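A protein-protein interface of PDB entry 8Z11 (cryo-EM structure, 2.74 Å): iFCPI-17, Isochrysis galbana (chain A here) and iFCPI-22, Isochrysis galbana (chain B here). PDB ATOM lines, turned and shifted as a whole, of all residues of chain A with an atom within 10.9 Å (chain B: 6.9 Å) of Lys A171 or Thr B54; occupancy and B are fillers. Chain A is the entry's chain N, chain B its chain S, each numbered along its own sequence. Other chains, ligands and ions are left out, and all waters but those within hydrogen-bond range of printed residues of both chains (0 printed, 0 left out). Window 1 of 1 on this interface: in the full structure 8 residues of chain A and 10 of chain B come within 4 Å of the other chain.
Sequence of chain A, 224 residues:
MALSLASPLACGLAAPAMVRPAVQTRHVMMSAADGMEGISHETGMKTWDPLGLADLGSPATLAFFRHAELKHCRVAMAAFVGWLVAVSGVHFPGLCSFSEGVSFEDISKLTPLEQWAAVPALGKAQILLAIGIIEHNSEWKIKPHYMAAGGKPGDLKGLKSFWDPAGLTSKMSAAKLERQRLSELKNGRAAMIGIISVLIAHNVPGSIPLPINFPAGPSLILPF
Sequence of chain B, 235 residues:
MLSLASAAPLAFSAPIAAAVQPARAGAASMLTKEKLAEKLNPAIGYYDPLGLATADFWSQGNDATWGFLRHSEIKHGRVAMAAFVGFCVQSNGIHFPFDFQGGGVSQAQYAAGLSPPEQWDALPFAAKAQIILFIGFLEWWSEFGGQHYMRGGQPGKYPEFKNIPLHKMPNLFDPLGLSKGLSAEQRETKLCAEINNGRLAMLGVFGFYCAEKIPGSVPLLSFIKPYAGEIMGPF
The backbone carbonyl oxygen of Gly A167 lies within hydrogen-bond range of the side-chain hydroxyl of Ser A170 (2.8 Å).
OD1 of Asp B48 sits close to N of Leu B50 (3.5 Å).
The backbone NH (N) of Gly B51 sits at hydrogen-bond distance from the side-chain carboxylate (OD1) of Asp B48 (2.7 Å).
N of Leu B52 is in hydrogen-bond range of OD2 of Asp B48 (3.0 Å).
O of Gly B51 sits at hydrogen-bond distance from OG1 of Thr B54, 3.2 Å away.
O of Ala B55 sits at hydrogen-bond distance from OG1 of Thr B65, 2.9 Å away.
Trp A163 touches none of the printed residues of chain B.
Printed residues of chain B within 4 Å of Gly A167: Gly B51 and Ala B55.
Of the printed residues of chain B, Leu A168 touches Leu B50.
Of the printed residues of chain B, Ser A170 touches Thr B54 (3.1 Å) and Ala B55 (3.9 Å).
Of chain B, only Pro B49 (2.8 Å), Leu B50 (3.8 Å) and Thr B54 (3.4 Å) come within 4 Å of Lys A171.
Of the printed residues of chain A, Leu B50 touches Leu A168 (3.1 Å) and Lys A171 (3.8 Å).
Printed residues of chain A within 4 Å of Gly B51: Gly A167 (3.6 Å).
No residue of chain A comes within 4 Å of Ala B53.
Of chain A, only Ser A170 (3.1 Å) and Lys A171 (3.4 Å) come within 4 Å of Thr B54.
Ala B55 touches just these residues of chain A: Ala A166 (3.0 Å), Gly A167 (3.7 Å) and Ser A170 (3.9 Å).
Of the printed residues of chain A, Asp B56 touches Pro A165 (3.6 Å).
No residue of chain A comes within 4 Å of Asn B62.
The nearest residue of chain A that does not touch Thr B54 is Gly A167 (4.6 Å).
Among the printed residues, merely in contact across the chains: Ala A166 with Ala B55, Leu A168 with Leu B50, Ser A170 with Thr B54, Ala A166 with Leu B52, Gly A167 with Gly B51, Pro A165 with Asp B56, Gly A167 with Ala B55, Lys A171 with Leu B50 and Ser A170 with Ala B55.
Hydrophobic or aromatic side chains of chain A that line the printed part of chain B: Leu A168.
Hydrophobic or aromatic side chains of chain B that line the printed part of chain A: Leu B50, Leu B52 and Ala B55.
Among the printed residues, no Asp or Glu carboxylate lies within 4 Å of a Lys or Arg side-chain nitrogen of the other chain.
The backbone carbonyl oxygen (O) of Pro B49 is in hydrogen-bond range of the side-chain amino group (NZ) of Lys A171 (2.8 Å).
The side-chain hydroxyl (OG1) of Thr B54 lies within hydrogen-bond range of the backbone NH (N) of Lys A171 (3.4 Å).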
ATOM      1  N   TRP A 163       0.757  15.231  34.730  1.00  0.00           N
ATOM      2  CA  TRP A 163       1.089  14.632  33.445  1.00  0.00           C
ATOM      3  C   TRP A 163      -0.130  14.663  32.538  1.00  0.00           C
ATOM      4  O   TRP A 163      -1.199  14.167  32.911  1.00  0.00           O
ATOM      5  CB  TRP A 163       1.559  13.189  33.599  1.00  0.00           C
ATOM      6  CG  TRP A 163       1.259  12.376  32.377  1.00  0.00           C
ATOM      7  CD1 TRP A 163       0.320  11.399  32.250  1.00  0.00           C
ATOM      8  CD2 TRP A 163       1.897  12.488  31.100  1.00  0.00           C
ATOM      9  NE1 TRP A 163       0.335  10.891  30.976  1.00  0.00           N
ATOM     10  CE2 TRP A 163       1.298  11.542  30.251  1.00  0.00           C
ATOM     11  CE3 TRP A 163       2.921  13.294  30.594  1.00  0.00           C
ATOM     12  CZ2 TRP A 163       1.682  11.385  28.924  1.00  0.00           C
ATOM     13  CZ3 TRP A 163       3.306  13.129  29.282  1.00  0.00           C
ATOM     14  CH2 TRP A 163       2.690  12.182  28.462  1.00  0.00           C
ATOM     15  N   ASP A 164       0.049  15.209  31.338  1.00  0.00           N
ATOM     16  CA  ASP A 164      -0.999  15.312  30.332  1.00  0.00           C
ATOM     17  C   ASP A 164      -2.242  15.960  30.926  1.00  0.00           C
ATOM     18  O   ASP A 164      -3.287  15.308  31.046  1.00  0.00           O
ATOM     19  CB  ASP A 164      -1.325  13.932  29.766  1.00  0.00           C
ATOM     20  CG  ASP A 164      -2.292  13.992  28.610  1.00  0.00           C
ATOM     21  OD1 ASP A 164      -2.108  14.851  27.723  1.00  0.00           O
ATOM     22  OD2 ASP A 164      -3.228  13.171  28.584  1.00  0.00           O
ATOM     23  N   PRO A 165      -2.163  17.225  31.341  1.00  0.00           N
ATOM     24  CA  PRO A 165      -3.362  17.884  31.867  1.00  0.00           C
ATOM     25  C   PRO A 165      -4.482  17.982  30.847  1.00  0.00           C
ATOM     26  O   PRO A 165      -5.658  17.956  31.228  1.00  0.00           O
ATOM     27  CB  PRO A 165      -2.840  19.267  32.285  1.00  0.00           C
ATOM     28  CG  PRO A 165      -1.375  19.174  32.276  1.00  0.00           C
ATOM     29  CD  PRO A 165      -1.042  18.169  31.241  1.00  0.00           C
ATOM     30  N   ALA A 166      -4.153  18.076  29.561  1.00  0.00           N
ATOM     31  CA  ALA A 166      -5.137  18.265  28.504  1.00  0.00           C
ATOM     32  C   ALA A 166      -5.715  16.959  27.971  1.00  0.00           C
ATOM     33  O   ALA A 166      -6.577  17.004  27.088  1.00  0.00           O
ATOM     34  CB  ALA A 166      -4.516  19.050  27.347  1.00  0.00           C
ATOM     35  N   GLY A 167      -5.266  15.810  28.462  1.00  0.00           N
ATOM     36  CA  GLY A 167      -5.856  14.547  28.049  1.00  0.00           C
ATOM     37  C   GLY A 167      -5.502  14.098  26.646  1.00  0.00           C
ATOM     38  O   GLY A 167      -6.273  13.349  26.032  1.00  0.00           O
ATOM     39  N   LEU A 168      -4.341  14.519  26.131  1.00  0.00           N
ATOM     40  CA  LEU A 168      -3.977  14.203  24.752  1.00  0.00           C
ATOM     41  C   LEU A 168      -3.893  12.699  24.529  1.00  0.00           C
ATOM     42  O   LEU A 168      -4.364  12.189  23.506  1.00  0.00           O
ATOM     43  CB  LEU A 168      -2.640  14.855  24.396  1.00  0.00           C
ATOM     44  CG  LEU A 168      -2.606  16.319  23.953  1.00  0.00           C
ATOM     45  CD1 LEU A 168      -1.176  16.734  23.662  1.00  0.00           C
ATOM     46  CD2 LEU A 168      -3.480  16.566  22.733  1.00  0.00           C
ATOM     47  N   THR A 169      -3.296  11.974  25.470  1.00  0.00           N
ATOM     48  CA  THR A 169      -3.191  10.523  25.352  1.00  0.00           C
ATOM     49  C   THR A 169      -4.518   9.806  25.575  1.00  0.00           C
ATOM     50  O   THR A 169      -4.607   8.607  25.283  1.00  0.00           O
ATOM     51  CB  THR A 169      -2.148   9.969  26.333  1.00  0.00           C
ATOM     52  OG1 THR A 169      -2.179   8.540  26.299  1.00  0.00           O
ATOM     53  CG2 THR A 169      -2.404  10.424  27.768  1.00  0.00           C
ATOM     54  N   SER A 170      -5.552  10.503  26.056  1.00  0.00           N
ATOM     55  CA  SER A 170      -6.827   9.861  26.357  1.00  0.00           C
ATOM     56  C   SER A 170      -7.480   9.225  25.136  1.00  0.00           C
ATOM     57  O   SER A 170      -8.319   8.334  25.302  1.00  0.00           O
ATOM     58  CB  SER A 170      -7.785  10.879  26.975  1.00  0.00           C
ATOM     59  OG  SER A 170      -7.143  11.624  27.994  1.00  0.00           O
ATOM     60  N   LYS A 171      -7.116   9.647  23.928  1.00  0.00           N
ATOM     61  CA  LYS A 171      -7.661   9.068  22.706  1.00  0.00           C
ATOM     62  C   LYS A 171      -7.041   7.723  22.351  1.00  0.00           C
ATOM     63  O   LYS A 171      -7.499   7.089  21.394  1.00  0.00           O
ATOM     64  CB  LYS A 171      -7.461  10.044  21.540  1.00  0.00           C
ATOM     65  CG  LYS A 171      -6.078   9.970  20.885  1.00  0.00           C
ATOM     66  CD  LYS A 171      -5.747  11.218  20.066  1.00  0.00           C
ATOM     67  CE  LYS A 171      -4.243  11.416  19.901  1.00  0.00           C
ATOM     68  NZ  LYS A 171      -3.904  12.807  19.495  1.00  0.00           N
ATOM     69  N   MET A 172      -6.026   7.270  23.085  1.00  0.00           N
ATOM     70  CA  MET A 172      -5.190   6.154  22.672  1.00  0.00           C
ATOM     71  C   MET A 172      -5.622   4.859  23.349  1.00  0.00           C
ATOM     72  O   MET A 172      -6.009   4.847  24.521  1.00  0.00           O
ATOM     73  CB  MET A 172      -3.722   6.438  22.989  1.00  0.00           C
ATOM     74  CG  MET A 172      -3.213   7.748  22.416  1.00  0.00           C
ATOM     75  SD  MET A 172      -1.529   8.125  22.907  1.00  0.00           S
ATOM     76  CE  MET A 172      -0.994   9.033  21.465  1.00  0.00           C
ATOM     77  N   SER A 173      -5.538   3.767  22.592  1.00  0.00           N
ATOM     78  CA  SER A 173      -5.895   2.442  23.074  1.00  0.00           C
ATOM     79  C   SER A 173      -4.681   1.789  23.736  1.00  0.00           C
ATOM     80  O   SER A 173      -3.637   2.416  23.925  1.00  0.00           O
ATOM     81  CB  SER A 173      -6.436   1.597  21.924  1.00  0.00           C
ATOM     82  OG  SER A 173      -5.394   1.205  21.047  1.00  0.00           O
ATOM     83  N   ALA A 174      -4.806   0.509  24.092  1.00  0.00           N
ATOM     84  CA  ALA A 174      -3.742  -0.166  24.830  1.00  0.00           C
ATOM     85  C   ALA A 174      -2.499  -0.357  23.969  1.00  0.00           C
ATOM     86  O   ALA A 174      -1.378  -0.079  24.411  1.00  0.00           O
ATOM     87  CB  ALA A 174      -4.243  -1.511  25.351  1.00  0.00           C
ATOM     88  N   ALA A 175      -2.673  -0.848  22.740  1.00  0.00           N
ATOM     89  CA  ALA A 175      -1.525  -1.071  21.867  1.00  0.00           C
ATOM     90  C   ALA A 175      -0.843   0.243  21.513  1.00  0.00           C
ATOM     91  O   ALA A 175       0.392   0.326  21.482  1.00  0.00           O
ATOM     92  CB  ALA A 175      -1.964  -1.805  20.601  1.00  0.00           C
ATOM     93  N   LYS A 176      -1.632   1.284  21.246  1.00  0.00           N
ATOM     94  CA  LYS A 176      -1.051   2.588  20.948  1.00  0.00           C
ATOM     95  C   LYS A 176      -0.314   3.145  22.157  1.00  0.00           C
ATOM     96  O   LYS A 176       0.751   3.753  22.014  1.00  0.00           O
ATOM     97  CB  LYS A 176      -2.134   3.566  20.487  1.00  0.00           C
ATOM     98  CG  LYS A 176      -1.836   4.243  19.161  1.00  0.00           C
ATOM     99  CD  LYS A 176      -0.688   5.233  19.278  1.00  0.00           C
ATOM    100  CE  LYS A 176      -0.259   5.741  17.913  1.00  0.00           C
ATOM    101  NZ  LYS A 176       1.003   6.523  17.981  1.00  0.00           N
ATOM    102  N   LEU A 177      -0.864   2.951  23.355  1.00  0.00           N
ATOM    103  CA  LEU A 177      -0.177   3.390  24.564  1.00  0.00           C
ATOM    104  C   LEU A 177       1.143   2.653  24.744  1.00  0.00           C
ATOM    105  O   LEU A 177       2.148   3.252  25.141  1.00  0.00           O
ATOM    106  CB  LEU A 177      -1.071   3.168  25.785  1.00  0.00           C
ATOM    107  CG  LEU A 177      -2.142   4.202  26.138  1.00  0.00           C
ATOM    108  CD1 LEU A 177      -2.877   3.765  27.396  1.00  0.00           C
ATOM    109  CD2 LEU A 177      -1.548   5.579  26.342  1.00  0.00           C
ATOM    110  N   GLU A 178       1.155   1.346  24.477  1.00  0.00           N
ATOM    111  CA  GLU A 178       2.390   0.578  24.591  1.00  0.00           C
ATOM    112  C   GLU A 178       3.425   1.083  23.593  1.00  0.00           C
ATOM    113  O   GLU A 178       4.608   1.238  23.932  1.00  0.00           O
ATOM    114  CB  GLU A 178       2.081  -0.910  24.387  1.00  0.00           C
ATOM    115  CG  GLU A 178       3.270  -1.885  24.271  1.00  0.00           C
ATOM    116  CD  GLU A 178       2.910  -3.134  23.488  1.00  0.00           C
ATOM    117  OE1 GLU A 178       3.249  -3.203  22.288  1.00  0.00           O
ATOM    118  OE2 GLU A 178       2.286  -4.045  24.071  1.00  0.00           O
ATOM    119  N   GLN A 180       3.579   4.107  22.333  1.00  0.00           N
ATOM    120  CA  GLN A 180       4.023   5.425  22.767  1.00  0.00           C
ATOM    121  C   GLN A 180       5.002   5.327  23.928  1.00  0.00           C
ATOM    122  O   GLN A 180       5.957   6.101  24.005  1.00  0.00           O
ATOM    123  CB  GLN A 180       2.827   6.292  23.157  1.00  0.00           C
ATOM    124  CG  GLN A 180       1.961   6.771  22.001  1.00  0.00           C
ATOM    125  CD  GLN A 180       2.710   7.658  21.032  1.00  0.00           C
ATOM    126  OE1 GLN A 180       3.456   7.174  20.187  1.00  0.00           O
ATOM    127  NE2 GLN A 180       2.531   8.965  21.165  1.00  0.00           N
ATOM    128  N   LYS B  33     -20.910  12.269  20.827  1.00  0.00           N
ATOM    129  CA  LYS B  33     -19.990  13.029  19.982  1.00  0.00           C
ATOM    130  C   LYS B  33     -20.165  12.649  18.519  1.00  0.00           C
ATOM    131  O   LYS B  33     -20.226  13.517  17.640  1.00  0.00           O
ATOM    132  CB  LYS B  33     -18.523  12.810  20.387  1.00  0.00           C
ATOM    133  CG  LYS B  33     -18.203  12.449  21.838  1.00  0.00           C
ATOM    134  CD  LYS B  33     -16.705  12.268  22.024  1.00  0.00           C
ATOM    135  CE  LYS B  33     -16.244  10.889  21.586  1.00  0.00           C
ATOM    136  NZ  LYS B  33     -14.783  10.698  21.797  1.00  0.00           N
ATOM    137  N   TYR B  46     -17.027  12.870  12.797  1.00  0.00           N
ATOM    138  CA  TYR B  46     -16.246  13.208  13.978  1.00  0.00           C
ATOM    139  C   TYR B  46     -14.790  13.435  13.594  1.00  0.00           C
ATOM    140  O   TYR B  46     -14.202  12.663  12.833  1.00  0.00           O
ATOM    141  CB  TYR B  46     -16.350  12.097  15.020  1.00  0.00           C
ATOM    142  CG  TYR B  46     -15.547  12.365  16.270  1.00  0.00           C
ATOM    143  CD1 TYR B  46     -16.039  13.185  17.270  1.00  0.00           C
ATOM    144  CD2 TYR B  46     -14.298  11.796  16.448  1.00  0.00           C
ATOM    145  CE1 TYR B  46     -15.308  13.431  18.411  1.00  0.00           C
ATOM    146  CE2 TYR B  46     -13.561  12.037  17.584  1.00  0.00           C
ATOM    147  CZ  TYR B  46     -14.071  12.854  18.563  1.00  0.00           C
ATOM    148  OH  TYR B  46     -13.336  13.097  19.698  1.00  0.00           O
ATOM    149  N   ASP B  48     -11.232  14.974  15.552  1.00  0.00           N
ATOM    150  CA  ASP B  48     -10.613  15.474  16.781  1.00  0.00           C
ATOM    151  C   ASP B  48      -9.176  14.978  16.833  1.00  0.00           C
ATOM    152  O   ASP B  48      -8.855  14.020  17.548  1.00  0.00           O
ATOM    153  CB  ASP B  48     -11.398  15.015  18.012  1.00  0.00           C
ATOM    154  CG  ASP B  48     -10.827  15.548  19.315  1.00  0.00           C
ATOM    155  OD1 ASP B  48      -9.896  16.378  19.284  1.00  0.00           O
ATOM    156  OD2 ASP B  48     -11.320  15.133  20.385  1.00  0.00           O
ATOM    157  N   PRO B  49      -8.274  15.598  16.061  1.00  0.00           N
ATOM    158  CA  PRO B  49      -6.865  15.165  16.103  1.00  0.00           C
ATOM    159  C   PRO B  49      -6.235  15.275  17.479  1.00  0.00           C
ATOM    160  O   PRO B  49      -5.442  14.407  17.863  1.00  0.00           O
ATOM    161  CB  PRO B  49      -6.173  16.094  15.097  1.00  0.00           C
ATOM    162  CG  PRO B  49      -7.240  16.701  14.291  1.00  0.00           C
ATOM    163  CD  PRO B  49      -8.506  16.656  15.064  1.00  0.00           C
ATOM    164  N   LEU B  50      -6.568  16.319  18.236  1.00  0.00           N
ATOM    165  CA  LEU B  50      -6.015  16.475  19.572  1.00  0.00           C
ATOM    166  C   LEU B  50      -6.620  15.500  20.572  1.00  0.00           C
ATOM    167  O   LEU B  50      -6.004  15.239  21.610  1.00  0.00           O
ATOM    168  CB  LEU B  50      -6.224  17.908  20.063  1.00  0.00           C
ATOM    169  CG  LEU B  50      -5.321  18.971  19.434  1.00  0.00           C
ATOM    170  CD1 LEU B  50      -5.902  20.356  19.656  1.00  0.00           C
ATOM    171  CD2 LEU B  50      -3.907  18.902  19.993  1.00  0.00           C
ATOM    172  N   GLY B  51      -7.794  14.951  20.283  1.00  0.00           N
ATOM    173  CA  GLY B  51      -8.446  14.046  21.211  1.00  0.00           C
ATOM    174  C   GLY B  51      -8.875  14.704  22.505  1.00  0.00           C
ATOM    175  O   GLY B  51      -8.773  14.086  23.571  1.00  0.00           O
ATOM    176  N   LEU B  52      -9.353  15.948  22.439  1.00  0.00           N
ATOM    177  CA  LEU B  52      -9.795  16.639  23.644  1.00  0.00           C
ATOM    178  C   LEU B  52     -11.167  16.178  24.113  1.00  0.00           C
ATOM    179  O   LEU B  52     -11.513  16.401  25.278  1.00  0.00           O
ATOM    180  CB  LEU B  52      -9.823  18.151  23.409  1.00  0.00           C
ATOM    181  CG  LEU B  52      -8.496  18.883  23.200  1.00  0.00           C
ATOM    182  CD1 LEU B  52      -8.764  20.358  22.982  1.00  0.00           C
ATOM    183  CD2 LEU B  52      -7.549  18.687  24.370  1.00  0.00           C
ATOM    184  N   ALA B  53     -11.959  15.549  23.241  1.00  0.00           N
ATOM    185  CA  ALA B  53     -13.283  15.095  23.650  1.00  0.00           C
ATOM    186  C   ALA B  53     -13.197  14.020  24.723  1.00  0.00           C
ATOM    187  O   ALA B  53     -14.072  13.939  25.591  1.00  0.00           O
ATOM    188  CB  ALA B  53     -14.055  14.573  22.443  1.00  0.00           C
ATOM    189  N   THR B  54     -12.157  13.192  24.681  1.00  0.00           N
ATOM    190  CA  THR B  54     -11.921  12.158  25.676  1.00  0.00           C
ATOM    191  C   THR B  54     -11.037  12.636  26.823  1.00  0.00           C
ATOM    192  O   THR B  54     -10.653  11.828  27.673  1.00  0.00           O
ATOM    193  CB  THR B  54     -11.285  10.935  25.015  1.00  0.00           C
ATOM    194  OG1 THR B  54     -10.058  11.317  24.384  1.00  0.00           O
ATOM    195  CG2 THR B  54     -12.217  10.342  23.973  1.00  0.00           C
ATOM    196  N   ALA B  55     -10.707  13.923  26.869  1.00  0.00           N
ATOM    197  CA  ALA B  55      -9.773  14.433  27.857  1.00  0.00           C
ATOM    198  C   ALA B  55     -10.403  14.459  29.245  1.00  0.00           C
ATOM    199  O   ALA B  55     -11.610  14.266  29.414  1.00  0.00           O
ATOM    200  CB  ALA B  55      -9.307  15.837  27.478  1.00  0.00           C
ATOM    201  N   ASP B  56      -9.556  14.688  30.246  1.00  0.00           N
ATOM    202  CA  ASP B  56      -9.962  14.832  31.642  1.00  0.00           C
ATOM    203  C   ASP B  56      -9.327  16.109  32.191  1.00  0.00           C
ATOM    204  O   ASP B  56      -8.266  16.078  32.819  1.00  0.00           O
ATOM    205  CB  ASP B  56      -9.544  13.555  32.459  1.00  0.00           C
ATOM    206  CG  ASP B  56     -10.511  13.217  33.584  1.00  0.00           C
ATOM    207  OD1 ASP B  56     -11.665  13.693  33.578  1.00  0.00           O
ATOM    208  OD2 ASP B  56     -10.108  12.454  34.487  1.00  0.00           O
ATOM    209  N   ASN B  62     -14.748  12.746  32.180  1.00  0.00           N
ATOM    210  CA  ASN B  62     -14.906  12.987  30.752  1.00  0.00           C
ATOM    211  C   ASN B  62     -16.236  13.647  30.432  1.00  0.00           C
ATOM    212  O   ASN B  62     -16.305  14.470  29.518  1.00  0.00           O
ATOM    213  CB  ASN B  62     -14.781  11.682  29.971  1.00  0.00           C
ATOM    214  CG  ASN B  62     -15.064  11.866  28.493  1.00  0.00           C
ATOM    215  OD1 ASN B  62     -15.819  11.098  27.897  1.00  0.00           O
ATOM    216  ND2 ASN B  62     -14.468  12.891  27.893  1.00  0.00           N
ATOM    217  N   THR B  65     -15.990  17.343  31.355  1.00  0.00           N
ATOM    218  CA  THR B  65     -15.031  18.042  30.509  1.00  0.00           C
ATOM    219  C   THR B  65     -15.547  18.169  29.080  1.00  0.00           C
ATOM    220  O   THR B  65     -15.298  19.177  28.409  1.00  0.00           O
ATOM    221  CB  THR B  65     -13.685  17.325  30.542  1.00  0.00           C
ATOM    222  OG1 THR B  65     -13.825  16.016  29.978  1.00  0.00           O
ATOM    223  CG2 THR B  65     -13.150  17.217  31.985  1.00  0.00           C
ATOM    224  N   TRP B  66     -16.282  17.163  28.604  1.00  0.00           N
ATOM    225  CA  TRP B  66     -16.944  17.268  27.311  1.00  0.00           C
ATOM    226  C   TRP B  66     -18.002  18.361  27.334  1.00  0.00           C
ATOM    227  O   TRP B  66     -18.158  19.107  26.359  1.00  0.00           O
ATOM    228  CB  TRP B  66     -17.560  15.917  26.949  1.00  0.00           C
ATOM    229  CG  TRP B  66     -18.443  15.927  25.747  1.00  0.00           C
ATOM    230  CD1 TRP B  66     -19.785  15.701  25.719  1.00  0.00           C
ATOM    231  CD2 TRP B  66     -18.047  16.160  24.393  1.00  0.00           C
ATOM    232  NE1 TRP B  66     -20.252  15.782  24.432  1.00  0.00           N
ATOM    233  CE2 TRP B  66     -19.202  16.065  23.599  1.00  0.00           C
ATOM    234  CE3 TRP B  66     -16.827  16.442  23.775  1.00  0.00           C
ATOM    235  CZ2 TRP B  66     -19.175  16.242  22.222  1.00  0.00           C
ATOM    236  CZ3 TRP B  66     -16.804  16.619  22.410  1.00  0.00           C
ATOM    237  CH2 TRP B  66     -17.971  16.518  21.648  1.00  0.00           C
ATOM    238  N   LEU B  69     -16.126  21.613  27.057  1.00  0.00           N
ATOM    239  CA  LEU B  69     -15.675  21.861  25.693  1.00  0.00           C
ATOM    240  C   LEU B  69     -16.828  22.299  24.800  1.00  0.00           C
ATOM    241  O   LEU B  69     -16.682  23.230  24.001  1.00  0.00           O
ATOM    242  CB  LEU B  69     -15.008  20.611  25.127  1.00  0.00           C
ATOM    243  CG  LEU B  69     -13.638  20.298  25.724  1.00  0.00           C
ATOM    244  CD1 LEU B  69     -13.345  18.818  25.626  1.00  0.00           C
ATOM    245  CD2 LEU B  69     -12.557  21.113  25.042  1.00  0.00           C
